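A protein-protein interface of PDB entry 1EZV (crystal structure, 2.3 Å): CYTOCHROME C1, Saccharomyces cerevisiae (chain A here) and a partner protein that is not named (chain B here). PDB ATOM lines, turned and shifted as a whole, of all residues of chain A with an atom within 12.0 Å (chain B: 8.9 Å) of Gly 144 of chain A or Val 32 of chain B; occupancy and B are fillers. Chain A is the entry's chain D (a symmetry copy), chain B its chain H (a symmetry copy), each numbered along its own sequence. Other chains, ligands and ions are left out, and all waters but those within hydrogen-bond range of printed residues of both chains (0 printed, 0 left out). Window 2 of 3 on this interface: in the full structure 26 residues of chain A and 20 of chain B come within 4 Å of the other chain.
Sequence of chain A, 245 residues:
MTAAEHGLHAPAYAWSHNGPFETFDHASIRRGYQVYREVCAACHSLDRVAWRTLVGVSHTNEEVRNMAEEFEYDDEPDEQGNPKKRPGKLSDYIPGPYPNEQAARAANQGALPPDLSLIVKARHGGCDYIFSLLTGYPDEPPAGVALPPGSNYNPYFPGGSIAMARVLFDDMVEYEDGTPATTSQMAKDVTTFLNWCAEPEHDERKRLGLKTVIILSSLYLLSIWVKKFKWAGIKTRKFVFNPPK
Of the printed residues of chain B, Ala 4 of chain A touches Val 51.
Of the printed residues of chain B, Pro 142 of chain A touches Tyr 25.
Of chain B, only Tyr 25 (3.1 Å), Ala 29 (3.7 Å), Asp 49 (3.3 Å) and Cys 50 (2.9 Å) come within 4 Å of Ala 143 of chain A.
Of chain B, only Val 32, Glu 48 and Asp 49 come within 4 Å of Gly 144 of chain A.
Printed residues of chain B within 4 Å of Val 145 of chain A: Val 51.
Gly 159 of chain A touches none of the printed residues of chain B.
Printed residues of chain A within 4 Å of Tyr 25 of chain B: Pro 142 and Ala 143.
No residue of chain A comes within 4 Å of Cys 28 of chain B.
Of chain A, only Ala 143 (3.7 Å) comes within 4 Å of Ala 29 of chain B.
No residue of chain A comes within 4 Å of Arg 31 of chain B.
Val 32 of chain B touches just one residue of chain A: Gly 144.
No residue of chain A comes within 4 Å of Lys 33 of chain B.
No residue of chain A comes within 4 Å of Gln 35 of chain B.
No residue of chain A comes within 4 Å of Gln 36 of chain B.
Of chain A, only Gly 144 comes within 4 Å of Glu 48 of chain B.
Asp 49 of chain B touches two residues of chain A.
Printed residues of chain A within 4 Å of Val 51 of chain B: Ala 4 and Val 145.
The nearest residue of chain B that does not touch Gly 144 of chain A is Gln 36 of chain B (4.4 Å).
The nearest residue of chain A that does not touch Val 32 of chain B is Ala 143 of chain A (4.1 Å).
The nearest printed residue of chain A that does not touch Tyr 25 of chain B is Pro 141 of chain A (4.4 Å).
The backbone NH (N) of Ala 143 of chain A is in hydrogen-bond range of the side-chain hydroxyl (OH) of Tyr 25 of chain B, 3.1 Å away.
N of Cys 50 of chain B sits at hydrogen-bond distance from O of Ala 143 of chain A (2.9 Å).
The side-chain sulfur (SG) of Cys 50 of chain B sits at hydrogen-bond distance from the backbone NH (N) of Ala 29 of chain B (3.6 Å).
O of Ala 4 of chain A lies within hydrogen-bond range of N of Gly 159 of chain A (2.8 Å).
The guanidinium group (NH1) of Arg 31 of chain B lies within salt-bridge range of the side-chain carboxylate (OE2) of Glu 48 of chain B.
N of Val 51 of chain B is in hydrogen-bond range of OD2 of Asp 49 of chain B, 3.2 Å away.
The side-chain carboxylate (OE1) of Glu 48 of chain B sits at hydrogen-bond distance from the side-chain amide nitrogen (NE2) of Gln 35 of chain B (3.5 Å).
The side-chain sulfur (SG) of Cys 50 of chain B forms a disulfide with the side-chain sulfur (SG) of Cys 28 of chain B (2.0 Å).
Printed residues of chain B that touch a printed residue of chain A: Tyr 25, Ala 29, Val 32, Glu 48, Asp 49, Cys 50 and Val 51.
Hydrophobic or aromatic side chains of chain B within 4 Å of the printed part of chain A: Tyr 25, Ala 29, Val 32 and Val 51.
Along chain B the printed residues that touch a printed residue of chain A span positions 25 to 51.
Of the 14 printed residues of chain A, 5 touch a printed residue of chain B.
Hydrophobic or aromatic side chains of chain A that line the printed part of chain B: Ala 4, Ala 143 and Val 145.
Among the printed residues, 10 pairs touch across the chains.
Among the printed residues, merely in contact across the chains: Ala 143 of chain A with Asp 49 of chain B (3.3 Å), Pro 142 of chain A with Tyr 25 of chain B (3.3 Å), Val 145 of chain A with Val 51 of chain B (3.6 Å), Ala 143 of chain A with Ala 29 of chain B (3.7 Å), Gly 144 of chain A with Val 32 of chain B (3.8 Å), Ala 4 of chain A with Val 51 of chain B (3.8 Å), Gly 144 of chain A with Asp 49 of chain B (3.9 Å) and Gly 144 of chain A with Glu 48 of chain B (3.9 Å).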
ATOM      1  N   ALA A   4      33.959 -41.698  29.423  1.00  0.00           N
ATOM      2  CA  ALA A   4      34.241 -41.499  28.005  1.00  0.00           C
ATOM      3  C   ALA A   4      35.496 -42.251  27.593  1.00  0.00           C
ATOM      4  O   ALA A   4      35.543 -42.864  26.526  1.00  0.00           O
ATOM      5  CB  ALA A   4      34.401 -40.013  27.708  1.00  0.00           C
ATOM      6  N   GLU A 140      24.244 -37.024  16.030  1.00  0.00           N
ATOM      7  CA  GLU A 140      25.124 -35.963  16.500  1.00  0.00           C
ATOM      8  C   GLU A 140      25.807 -36.363  17.809  1.00  0.00           C
ATOM      9  O   GLU A 140      25.205 -37.034  18.647  1.00  0.00           O
ATOM     10  CB  GLU A 140      24.327 -34.664  16.685  1.00  0.00           C
ATOM     11  CG  GLU A 140      24.374 -33.730  15.472  1.00  0.00           C
ATOM     12  CD  GLU A 140      23.145 -32.839  15.364  1.00  0.00           C
ATOM     13  OE1 GLU A 140      23.208 -31.673  15.818  1.00  0.00           O
ATOM     14  OE2 GLU A 140      22.123 -33.301  14.806  1.00  0.00           O
ATOM     15  N   PRO A 141      27.092 -35.998  17.977  1.00  0.00           N
ATOM     16  CA  PRO A 141      27.803 -36.146  19.252  1.00  0.00           C
ATOM     17  C   PRO A 141      27.143 -35.369  20.391  1.00  0.00           C
ATOM     18  O   PRO A 141      26.530 -34.327  20.164  1.00  0.00           O
ATOM     19  CB  PRO A 141      29.206 -35.613  18.942  1.00  0.00           C
ATOM     20  CG  PRO A 141      29.016 -34.725  17.760  1.00  0.00           C
ATOM     21  CD  PRO A 141      27.967 -35.418  16.944  1.00  0.00           C
ATOM     22  N   PRO A 142      27.267 -35.869  21.636  1.00  0.00           N
ATOM     23  CA  PRO A 142      26.809 -35.131  22.816  1.00  0.00           C
ATOM     24  C   PRO A 142      27.433 -33.741  22.912  1.00  0.00           C
ATOM     25  O   PRO A 142      28.561 -33.520  22.467  1.00  0.00           O
ATOM     26  CB  PRO A 142      27.225 -36.028  23.986  1.00  0.00           C
ATOM     27  CG  PRO A 142      28.324 -36.867  23.443  1.00  0.00           C
ATOM     28  CD  PRO A 142      27.935 -37.124  22.019  1.00  0.00           C
ATOM     29  N   ALA A 143      26.675 -32.811  23.482  1.00  0.00           N
ATOM     30  CA  ALA A 143      27.061 -31.408  23.518  1.00  0.00           C
ATOM     31  C   ALA A 143      28.392 -31.203  24.230  1.00  0.00           C
ATOM     32  O   ALA A 143      28.613 -31.741  25.314  1.00  0.00           O
ATOM     33  CB  ALA A 143      25.974 -30.593  24.197  1.00  0.00           C
ATOM     34  N   GLY A 144      29.286 -30.455  23.590  1.00  0.00           N
ATOM     35  CA  GLY A 144      30.551 -30.114  24.212  1.00  0.00           C
ATOM     36  C   GLY A 144      31.704 -30.932  23.674  1.00  0.00           C
ATOM     37  O   GLY A 144      32.862 -30.523  23.766  1.00  0.00           O
ATOM     38  N   VAL A 145      31.382 -32.093  23.110  1.00  0.00           N
ATOM     39  CA  VAL A 145      32.388 -32.972  22.530  1.00  0.00           C
ATOM     40  C   VAL A 145      32.896 -32.406  21.205  1.00  0.00           C
ATOM     41  O   VAL A 145      32.129 -32.231  20.252  1.00  0.00           O
ATOM     42  CB  VAL A 145      31.825 -34.396  22.305  1.00  0.00           C
ATOM     43  CG1 VAL A 145      32.895 -35.298  21.720  1.00  0.00           C
ATOM     44  CG2 VAL A 145      31.329 -34.968  23.617  1.00  0.00           C
ATOM     45  N   ALA A 146      34.174 -32.039  21.194  1.00  0.00           N
ATOM     46  CA  ALA A 146      34.829 -31.527  19.998  1.00  0.00           C
ATOM     47  C   ALA A 146      35.572 -32.654  19.295  1.00  0.00           C
ATOM     48  O   ALA A 146      36.629 -33.101  19.750  1.00  0.00           O
ATOM     49  CB  ALA A 146      35.796 -30.404  20.368  1.00  0.00           C
ATOM     50  N   LEU A 147      34.987 -33.131  18.201  1.00  0.00           N
ATOM     51  CA  LEU A 147      35.534 -34.245  17.436  1.00  0.00           C
ATOM     52  C   LEU A 147      36.604 -33.761  16.464  1.00  0.00           C
ATOM     53  O   LEU A 147      36.367 -32.836  15.685  1.00  0.00           O
ATOM     54  CB  LEU A 147      34.411 -34.930  16.658  1.00  0.00           C
ATOM     55  CG  LEU A 147      34.206 -36.434  16.842  1.00  0.00           C
ATOM     56  CD1 LEU A 147      34.362 -36.841  18.305  1.00  0.00           C
ATOM     57  CD2 LEU A 147      32.821 -36.782  16.328  1.00  0.00           C
ATOM     58  N   PRO A 148      37.780 -34.417  16.459  1.00  0.00           N
ATOM     59  CA  PRO A 148      38.801 -34.194  15.427  1.00  0.00           C
ATOM     60  C   PRO A 148      38.241 -34.333  14.008  1.00  0.00           C
ATOM     61  O   PRO A 148      37.284 -35.076  13.778  1.00  0.00           O
ATOM     62  CB  PRO A 148      39.851 -35.264  15.730  1.00  0.00           C
ATOM     63  CG  PRO A 148      39.699 -35.520  17.190  1.00  0.00           C
ATOM     64  CD  PRO A 148      38.219 -35.421  17.444  1.00  0.00           C
ATOM     65  N   TYR A 153      31.962 -40.041  16.157  1.00  0.00           N
ATOM     66  CA  TYR A 153      31.646 -40.355  17.536  1.00  0.00           C
ATOM     67  C   TYR A 153      30.866 -41.652  17.650  1.00  0.00           C
ATOM     68  O   TYR A 153      29.944 -41.912  16.876  1.00  0.00           O
ATOM     69  CB  TYR A 153      30.864 -39.222  18.193  1.00  0.00           C
ATOM     70  CG  TYR A 153      30.593 -39.456  19.662  1.00  0.00           C
ATOM     71  CD1 TYR A 153      31.545 -39.132  20.627  1.00  0.00           C
ATOM     72  CD2 TYR A 153      29.403 -40.048  20.081  1.00  0.00           C
ATOM     73  CE1 TYR A 153      31.317 -39.392  21.978  1.00  0.00           C
ATOM     74  CE2 TYR A 153      29.169 -40.325  21.422  1.00  0.00           C
ATOM     75  CZ  TYR A 153      30.129 -39.991  22.361  1.00  0.00           C
ATOM     76  OH  TYR A 153      29.878 -40.236  23.683  1.00  0.00           O
ATOM     77  N   GLY A 159      37.173 -43.740  24.424  1.00  0.00           N
ATOM     78  CA  GLY A 159      37.547 -42.389  24.032  1.00  0.00           C
ATOM     79  C   GLY A 159      36.556 -41.720  23.092  1.00  0.00           C
ATOM     80  O   GLY A 159      36.736 -40.554  22.732  1.00  0.00           O
ATOM     81  N   GLY A 160      35.594 -42.499  22.595  1.00  0.00           N
ATOM     82  CA  GLY A 160      34.477 -41.950  21.845  1.00  0.00           C
ATOM     83  C   GLY A 160      34.758 -41.623  20.388  1.00  0.00           C
ATOM     84  O   GLY A 160      33.837 -41.585  19.569  1.00  0.00           O
ATOM     85  N   SER A 161      36.028 -41.412  20.060  1.00  0.00           N
ATOM     86  CA  SER A 161      36.411 -40.933  18.742  1.00  0.00           C
ATOM     87  C   SER A 161      36.981 -42.056  17.865  1.00  0.00           C
ATOM     88  O   SER A 161      38.132 -42.462  18.023  1.00  0.00           O
ATOM     89  CB  SER A 161      37.418 -39.792  18.901  1.00  0.00           C
ATOM     90  OG  SER A 161      38.029 -39.460  17.671  1.00  0.00           O
ATOM     91  N   TYR B  25      19.809 -34.574  30.150  1.00  0.00           N
ATOM     92  CA  TYR B  25      20.776 -34.431  29.067  1.00  0.00           C
ATOM     93  C   TYR B  25      20.554 -33.106  28.350  1.00  0.00           C
ATOM     94  O   TYR B  25      21.513 -32.432  27.968  1.00  0.00           O
ATOM     95  CB  TYR B  25      20.668 -35.593  28.064  1.00  0.00           C
ATOM     96  CG  TYR B  25      21.490 -35.373  26.807  1.00  0.00           C
ATOM     97  CD1 TYR B  25      22.882 -35.353  26.867  1.00  0.00           C
ATOM     98  CD2 TYR B  25      20.881 -34.956  25.620  1.00  0.00           C
ATOM     99  CE1 TYR B  25      23.647 -34.899  25.799  1.00  0.00           C
ATOM    100  CE2 TYR B  25      21.639 -34.497  24.538  1.00  0.00           C
ATOM    101  CZ  TYR B  25      23.024 -34.466  24.639  1.00  0.00           C
ATOM    102  OH  TYR B  25      23.782 -33.953  23.607  1.00  0.00           O
ATOM    103  N   GLU B  26      19.285 -32.736  28.183  1.00  0.00           N
ATOM    104  CA  GLU B  26      18.915 -31.510  27.475  1.00  0.00           C
ATOM    105  C   GLU B  26      19.304 -30.275  28.272  1.00  0.00           C
ATOM    106  O   GLU B  26      19.848 -29.319  27.719  1.00  0.00           O
ATOM    107  CB  GLU B  26      17.412 -31.485  27.204  1.00  0.00           C
ATOM    108  CG  GLU B  26      17.057 -31.021  25.810  1.00  0.00           C
ATOM    109  CD  GLU B  26      17.086 -32.147  24.799  1.00  0.00           C
ATOM    110  OE1 GLU B  26      18.149 -32.356  24.169  1.00  0.00           O
ATOM    111  OE2 GLU B  26      16.042 -32.817  24.632  1.00  0.00           O
ATOM    112  N   GLU B  27      19.041 -30.316  29.575  1.00  0.00           N
ATOM    113  CA  GLU B  27      19.442 -29.248  30.484  1.00  0.00           C
ATOM    114  C   GLU B  27      20.960 -29.056  30.489  1.00  0.00           C
ATOM    115  O   GLU B  27      21.449 -27.944  30.695  1.00  0.00           O
ATOM    116  CB  GLU B  27      18.946 -29.549  31.899  1.00  0.00           C
ATOM    117  CG  GLU B  27      18.873 -28.328  32.804  1.00  0.00           C
ATOM    118  CD  GLU B  27      17.854 -28.489  33.919  1.00  0.00           C
ATOM    119  OE1 GLU B  27      18.253 -28.897  35.035  1.00  0.00           O
ATOM    120  OE2 GLU B  27      16.654 -28.219  33.672  1.00  0.00           O
ATOM    121  N   CYS B  28      21.696 -30.135  30.222  1.00  0.00           N
ATOM    122  CA  CYS B  28      23.145 -30.058  30.083  1.00  0.00           C
ATOM    123  C   CYS B  28      23.532 -29.405  28.762  1.00  0.00           C
ATOM    124  O   CYS B  28      24.407 -28.542  28.726  1.00  0.00           O
ATOM    125  CB  CYS B  28      23.776 -31.453  30.172  1.00  0.00           C
ATOM    126  SG  CYS B  28      25.602 -31.443  30.169  1.00  0.00           S
ATOM    127  N   ALA B  29      22.874 -29.824  27.683  1.00  0.00           N
ATOM    128  CA  ALA B  29      23.168 -29.332  26.339  1.00  0.00           C
ATOM    129  C   ALA B  29      22.926 -27.827  26.201  1.00  0.00           C
ATOM    130  O   ALA B  29      23.681 -27.125  25.523  1.00  0.00           O
ATOM    131  CB  ALA B  29      22.333 -30.094  25.316  1.00  0.00           C
ATOM    132  N   GLU B  30      21.862 -27.350  26.842  1.00  0.00           N
ATOM    133  CA  GLU B  30      21.557 -25.923  26.911  1.00  0.00           C
ATOM    134  C   GLU B  30      22.694 -25.167  27.593  1.00  0.00           C
ATOM    135  O   GLU B  30      23.271 -24.241  27.018  1.00  0.00           O
ATOM    136  CB  GLU B  30      20.252 -25.712  27.688  1.00  0.00           C
ATOM    137  CG  GLU B  30      19.719 -24.283  27.671  1.00  0.00           C
ATOM    138  CD  GLU B  30      18.246 -24.201  28.051  1.00  0.00           C
ATOM    139  OE1 GLU B  30      17.889 -24.615  29.179  1.00  0.00           O
ATOM    140  OE2 GLU B  30      17.448 -23.722  27.216  1.00  0.00           O
ATOM    141  N   ARG B  31      23.068 -25.642  28.778  1.00  0.00           N
ATOM    142  CA  ARG B  31      24.128 -25.040  29.581  1.00  0.00           C
ATOM    143  C   ARG B  31      25.443 -24.919  28.809  1.00  0.00           C
ATOM    144  O   ARG B  31      26.174 -23.942  28.969  1.00  0.00           O
ATOM    145  CB  ARG B  31      24.328 -25.871  30.854  1.00  0.00           C
ATOM    146  CG  ARG B  31      25.223 -25.237  31.904  1.00  0.00           C
ATOM    147  CD  ARG B  31      25.028 -25.894  33.271  1.00  0.00           C
ATOM    148  NE  ARG B  31      25.412 -27.306  33.284  1.00  0.00           N
ATOM    149  CZ  ARG B  31      24.573 -28.313  33.518  1.00  0.00           C
ATOM    150  NH1 ARG B  31      25.018 -29.564  33.516  1.00  0.00           N
ATOM    151  NH2 ARG B  31      23.285 -28.076  33.733  1.00  0.00           N
ATOM    152  N   VAL B  32      25.678 -25.849  27.887  1.00  0.00           N
ATOM    153  CA  VAL B  32      26.934 -25.901  27.146  1.00  0.00           C
ATOM    154  C   VAL B  32      26.990 -24.899  25.994  1.00  0.00           C
ATOM    155  O   VAL B  32      27.983 -24.188  25.843  1.00  0.00           O
ATOM    156  CB  VAL B  32      27.206 -27.330  26.610  1.00  0.00           C
ATOM    157  CG1 VAL B  32      28.437 -27.342  25.710  1.00  0.00           C
ATOM    158  CG2 VAL B  32      27.412 -28.283  27.770  1.00  0.00           C
ATOM    159  N   LYS B  33      25.925 -24.826  25.195  1.00  0.00           N
ATOM    160  CA  LYS B  33      25.903 -23.928  24.038  1.00  0.00           C
ATOM    161  C   LYS B  33      25.931 -22.457  24.458  1.00  0.00           C
ATOM    162  O   LYS B  33      26.412 -21.600  23.716  1.00  0.00           O
ATOM    163  CB  LYS B  33      24.680 -24.207  23.151  1.00  0.00           C
ATOM    164  CG  LYS B  33      23.364 -23.624  23.651  1.00  0.00           C
ATOM    165  CD  LYS B  33      22.368 -23.459  22.509  1.00  0.00           C
ATOM    166  CE  LYS B  33      21.003 -23.002  23.010  1.00  0.00           C
ATOM    167  NZ  LYS B  33      20.293 -24.063  23.789  1.00  0.00           N
ATOM    168  N   ILE B  34      25.459 -22.189  25.673  1.00  0.00           N
ATOM    169  CA  ILE B  34      25.540 -20.862  26.274  1.00  0.00           C
ATOM    170  C   ILE B  34      26.991 -20.521  26.615  1.00  0.00           C
ATOM    171  O   ILE B  34      27.438 -19.394  26.398  1.00  0.00           O
ATOM    172  CB  ILE B  34      24.669 -20.784  27.558  1.00  0.00           C
ATOM    173  CG1 ILE B  34      23.185 -20.834  27.182  1.00  0.00           C
ATOM    174  CG2 ILE B  34      24.970 -19.509  28.339  1.00  0.00           C
ATOM    175  CD1 ILE B  34      22.253 -20.967  28.367  1.00  0.00           C
ATOM    176  N   GLN B  35      27.731 -21.514  27.100  1.00  0.00           N
ATOM    177  CA  GLN B  35      29.137 -21.334  27.456  1.00  0.00           C
ATOM    178  C   GLN B  35      30.013 -21.075  26.230  1.00  0.00           C
ATOM    179  O   GLN B  35      31.049 -20.415  26.329  1.00  0.00           O
ATOM    180  CB  GLN B  35      29.658 -22.566  28.202  1.00  0.00           C
ATOM    181  CG  GLN B  35      29.182 -22.690  29.640  1.00  0.00           C
ATOM    182  CD  GLN B  35      29.761 -23.907  30.347  1.00  0.00           C
ATOM    183  OE1 GLN B  35      30.833 -24.399  29.988  1.00  0.00           O
ATOM    184  NE2 GLN B  35      29.054 -24.393  31.362  1.00  0.00           N
ATOM    185  N   GLN B  36      29.589 -21.594  25.079  1.00  0.00           N
ATOM    186  CA  GLN B  36      30.359 -21.484  23.840  1.00  0.00           C
ATOM    187  C   GLN B  36      30.244 -20.098  23.207  1.00  0.00           C
ATOM    188  O   GLN B  36      31.119 -19.679  22.447  1.00  0.00           O
ATOM    189  CB  GLN B  36      29.903 -22.547  22.836  1.00  0.00           C
ATOM    190  CG  GLN B  36      29.984 -23.975  23.358  1.00  0.00           C
ATOM    191  CD  GLN B  36      29.741 -25.016  22.282  1.00  0.00           C
ATOM    192  OE1 GLN B  36      30.304 -26.108  22.324  1.00  0.00           O
ATOM    193  NE2 GLN B  36      28.886 -24.689  21.318  1.00  0.00           N
ATOM    194  N   GLN B  37      29.166 -19.392  23.537  1.00  0.00           N
ATOM    195  CA  GLN B  37      28.908 -18.061  22.994  1.00  0.00           C
ATOM    196  C   GLN B  37      29.220 -16.962  24.011  1.00  0.00           C
ATOM    197  O   GLN B  37      28.590 -15.903  24.012  1.00  0.00           O
ATOM    198  CB  GLN B  37      27.451 -17.958  22.542  1.00  0.00           C
ATOM    199  CG  GLN B  37      27.102 -18.869  21.381  1.00  0.00           C
ATOM    200  CD  GLN B  37      25.613 -18.920  21.102  1.00  0.00           C
ATOM    201  OE1 GLN B  37      24.816 -18.273  21.785  1.00  0.00           O
ATOM    202  NE2 GLN B  37      25.227 -19.701  20.099  1.00  0.00           N
ATOM    203  N   GLN B  38      30.173 -17.239  24.895  1.00  0.00           N
ATOM    204  CA  GLN B  38      30.663 -16.249  25.847  1.00  0.00           C
ATOM    205  C   GLN B  38      32.188 -16.255  25.819  1.00  0.00           C
ATOM    206  O   GLN B  38      32.809 -17.315  25.905  1.00  0.00           O
ATOM    207  CB  GLN B  38      30.164 -16.569  27.260  1.00  0.00           C
ATOM    208  CG  GLN B  38      28.650 -16.511  27.416  1.00  0.00           C
ATOM    209  CD  GLN B  38      28.198 -16.598  28.863  1.00  0.00           C
ATOM    210  OE1 GLN B  38      27.215 -15.968  29.254  1.00  0.00           O
ATOM    211  NE2 GLN B  38      28.905 -17.390  29.663  1.00  0.00           N
ATOM    212  N   TYR B  41      36.171 -18.932  25.247  1.00  0.00           N
ATOM    213  CA  TYR B  41      35.834 -20.351  25.251  1.00  0.00           C
ATOM    214  C   TYR B  41      36.984 -21.189  24.705  1.00  0.00           C
ATOM    215  O   TYR B  41      37.307 -22.242  25.256  1.00  0.00           O
ATOM    216  CB  TYR B  41      34.570 -20.605  24.427  1.00  0.00           C
ATOM    217  CG  TYR B  41      34.092 -22.039  24.479  1.00  0.00           C
ATOM    218  CD1 TYR B  41      34.136 -22.850  23.346  1.00  0.00           C
ATOM    219  CD2 TYR B  41      33.641 -22.600  25.674  1.00  0.00           C
ATOM    220  CE1 TYR B  41      33.746 -24.187  23.401  1.00  0.00           C
ATOM    221  CE2 TYR B  41      33.249 -23.934  25.741  1.00  0.00           C
ATOM    222  CZ  TYR B  41      33.304 -24.723  24.600  1.00  0.00           C
ATOM    223  OH  TYR B  41      32.915 -26.041  24.656  1.00  0.00           O
ATOM    224  N   LEU B  44      39.931 -21.794  27.929  1.00  0.00           N
ATOM    225  CA  LEU B  44      39.263 -21.956  29.219  1.00  0.00           C
ATOM    226  C   LEU B  44      39.798 -23.125  30.047  1.00  0.00           C
ATOM    227  O   LEU B  44      39.685 -23.114  31.275  1.00  0.00           O
ATOM    228  CB  LEU B  44      37.752 -22.117  29.016  1.00  0.00           C
ATOM    229  CG  LEU B  44      36.838 -21.195  29.832  1.00  0.00           C
ATOM    230  CD1 LEU B  44      35.426 -21.259  29.276  1.00  0.00           C
ATOM    231  CD2 LEU B  44      36.848 -21.594  31.298  1.00  0.00           C
ATOM    232  N   LYS B  47      36.256 -26.782  29.856  1.00  0.00           N
ATOM    233  CA  LYS B  47      35.049 -26.909  29.044  1.00  0.00           C
ATOM    234  C   LYS B  47      34.226 -28.123  29.465  1.00  0.00           C
ATOM    235  O   LYS B  47      34.736 -29.243  29.530  1.00  0.00           O
ATOM    236  CB  LYS B  47      35.416 -27.028  27.562  1.00  0.00           C
ATOM    237  CG  LYS B  47      36.414 -25.985  27.069  1.00  0.00           C
ATOM    238  CD  LYS B  47      36.835 -26.260  25.630  1.00  0.00           C
ATOM    239  CE  LYS B  47      38.329 -26.025  25.424  1.00  0.00           C
ATOM    240  NZ  LYS B  47      38.691 -24.581  25.416  1.00  0.00           N
ATOM    241  N   GLU B  48      32.956 -27.887  29.770  1.00  0.00           N
ATOM    242  CA  GLU B  48      32.046 -28.955  30.155  1.00  0.00           C
ATOM    243  C   GLU B  48      31.452 -29.622  28.919  1.00  0.00           C
ATOM    244  O   GLU B  48      31.158 -28.956  27.922  1.00  0.00           O
ATOM    245  CB  GLU B  48      30.924 -28.400  31.034  1.00  0.00           C
ATOM    246  CG  GLU B  48      29.993 -29.465  31.605  1.00  0.00           C
ATOM    247  CD  GLU B  48      28.837 -28.888  32.406  1.00  0.00           C
ATOM    248  OE1 GLU B  48      28.711 -27.646  32.488  1.00  0.00           O
ATOM    249  OE2 GLU B  48      28.043 -29.682  32.955  1.00  0.00           O
ATOM    250  N   ASP B  49      31.358 -30.949  28.960  1.00  0.00           N
ATOM    251  CA  ASP B  49      30.620 -31.700  27.952  1.00  0.00           C
ATOM    252  C   ASP B  49      29.491 -32.479  28.608  1.00  0.00           C
ATOM    253  O   ASP B  49      29.358 -32.478  29.826  1.00  0.00           O
ATOM    254  CB  ASP B  49      31.549 -32.648  27.179  1.00  0.00           C
ATOM    255  CG  ASP B  49      32.269 -33.638  28.081  1.00  0.00           C
ATOM    256  OD1 ASP B  49      33.516 -33.559  28.154  1.00  0.00           O
ATOM    257  OD2 ASP B  49      31.604 -34.522  28.670  1.00  0.00           O
ATOM    258  N   CYS B  50      28.691 -33.163  27.801  1.00  0.00           N
ATOM    259  CA  CYS B  50      27.517 -33.845  28.319  1.00  0.00           C
ATOM    260  C   CYS B  50      27.541 -35.352  28.045  1.00  0.00           C
ATOM    261  O   CYS B  50      26.492 -36.010  28.032  1.00  0.00           O
ATOM    262  CB  CYS B  50      26.254 -33.189  27.749  1.00  0.00           C
ATOM    263  SG  CYS B  50      26.096 -31.422  28.193  1.00  0.00           S
ATOM    264  N   VAL B  51      28.755 -35.906  27.982  1.00  0.00           N
ATOM    265  CA  VAL B  51      28.960 -37.343  27.787  1.00  0.00           C
ATOM    266  C   VAL B  51      28.324 -38.144  28.920  1.00  0.00           C
ATOM    267  O   VAL B  51      27.559 -39.071  28.680  1.00  0.00           O
ATOM    268  CB  VAL B  51      30.466 -37.693  27.707  1.00  0.00           C
ATOM    269  CG1 VAL B  51      30.656 -39.196  27.588  1.00  0.00           C
ATOM    270  CG2 VAL B  51      31.101 -37.010  26.518  1.00  0.00           C
ATOM    271  N   GLU B  53      25.836 -37.376  31.038  1.00  0.00           N
ATOM    272  CA  GLU B  53      24.378 -37.354  30.931  1.00  0.00           C
ATOM    273  C   GLU B  53      23.907 -38.155  29.724  1.00  0.00           C
ATOM    274  O   GLU B  53      22.908 -38.873  29.800  1.00  0.00           O
ATOM    275  CB  GLU B  53      23.869 -35.912  30.824  1.00  0.00           C
ATOM    276  CG  GLU B  53      24.019 -35.087  32.100  1.00  0.00           C
ATOM    277  CD  GLU B  53      25.414 -34.508  32.282  1.00  0.00           C
ATOM    278  OE1 GLU B  53      26.224 -34.561  31.330  1.00  0.00           O
ATOM    279  OE2 GLU B  53      25.695 -33.983  33.381  1.00  0.00           O
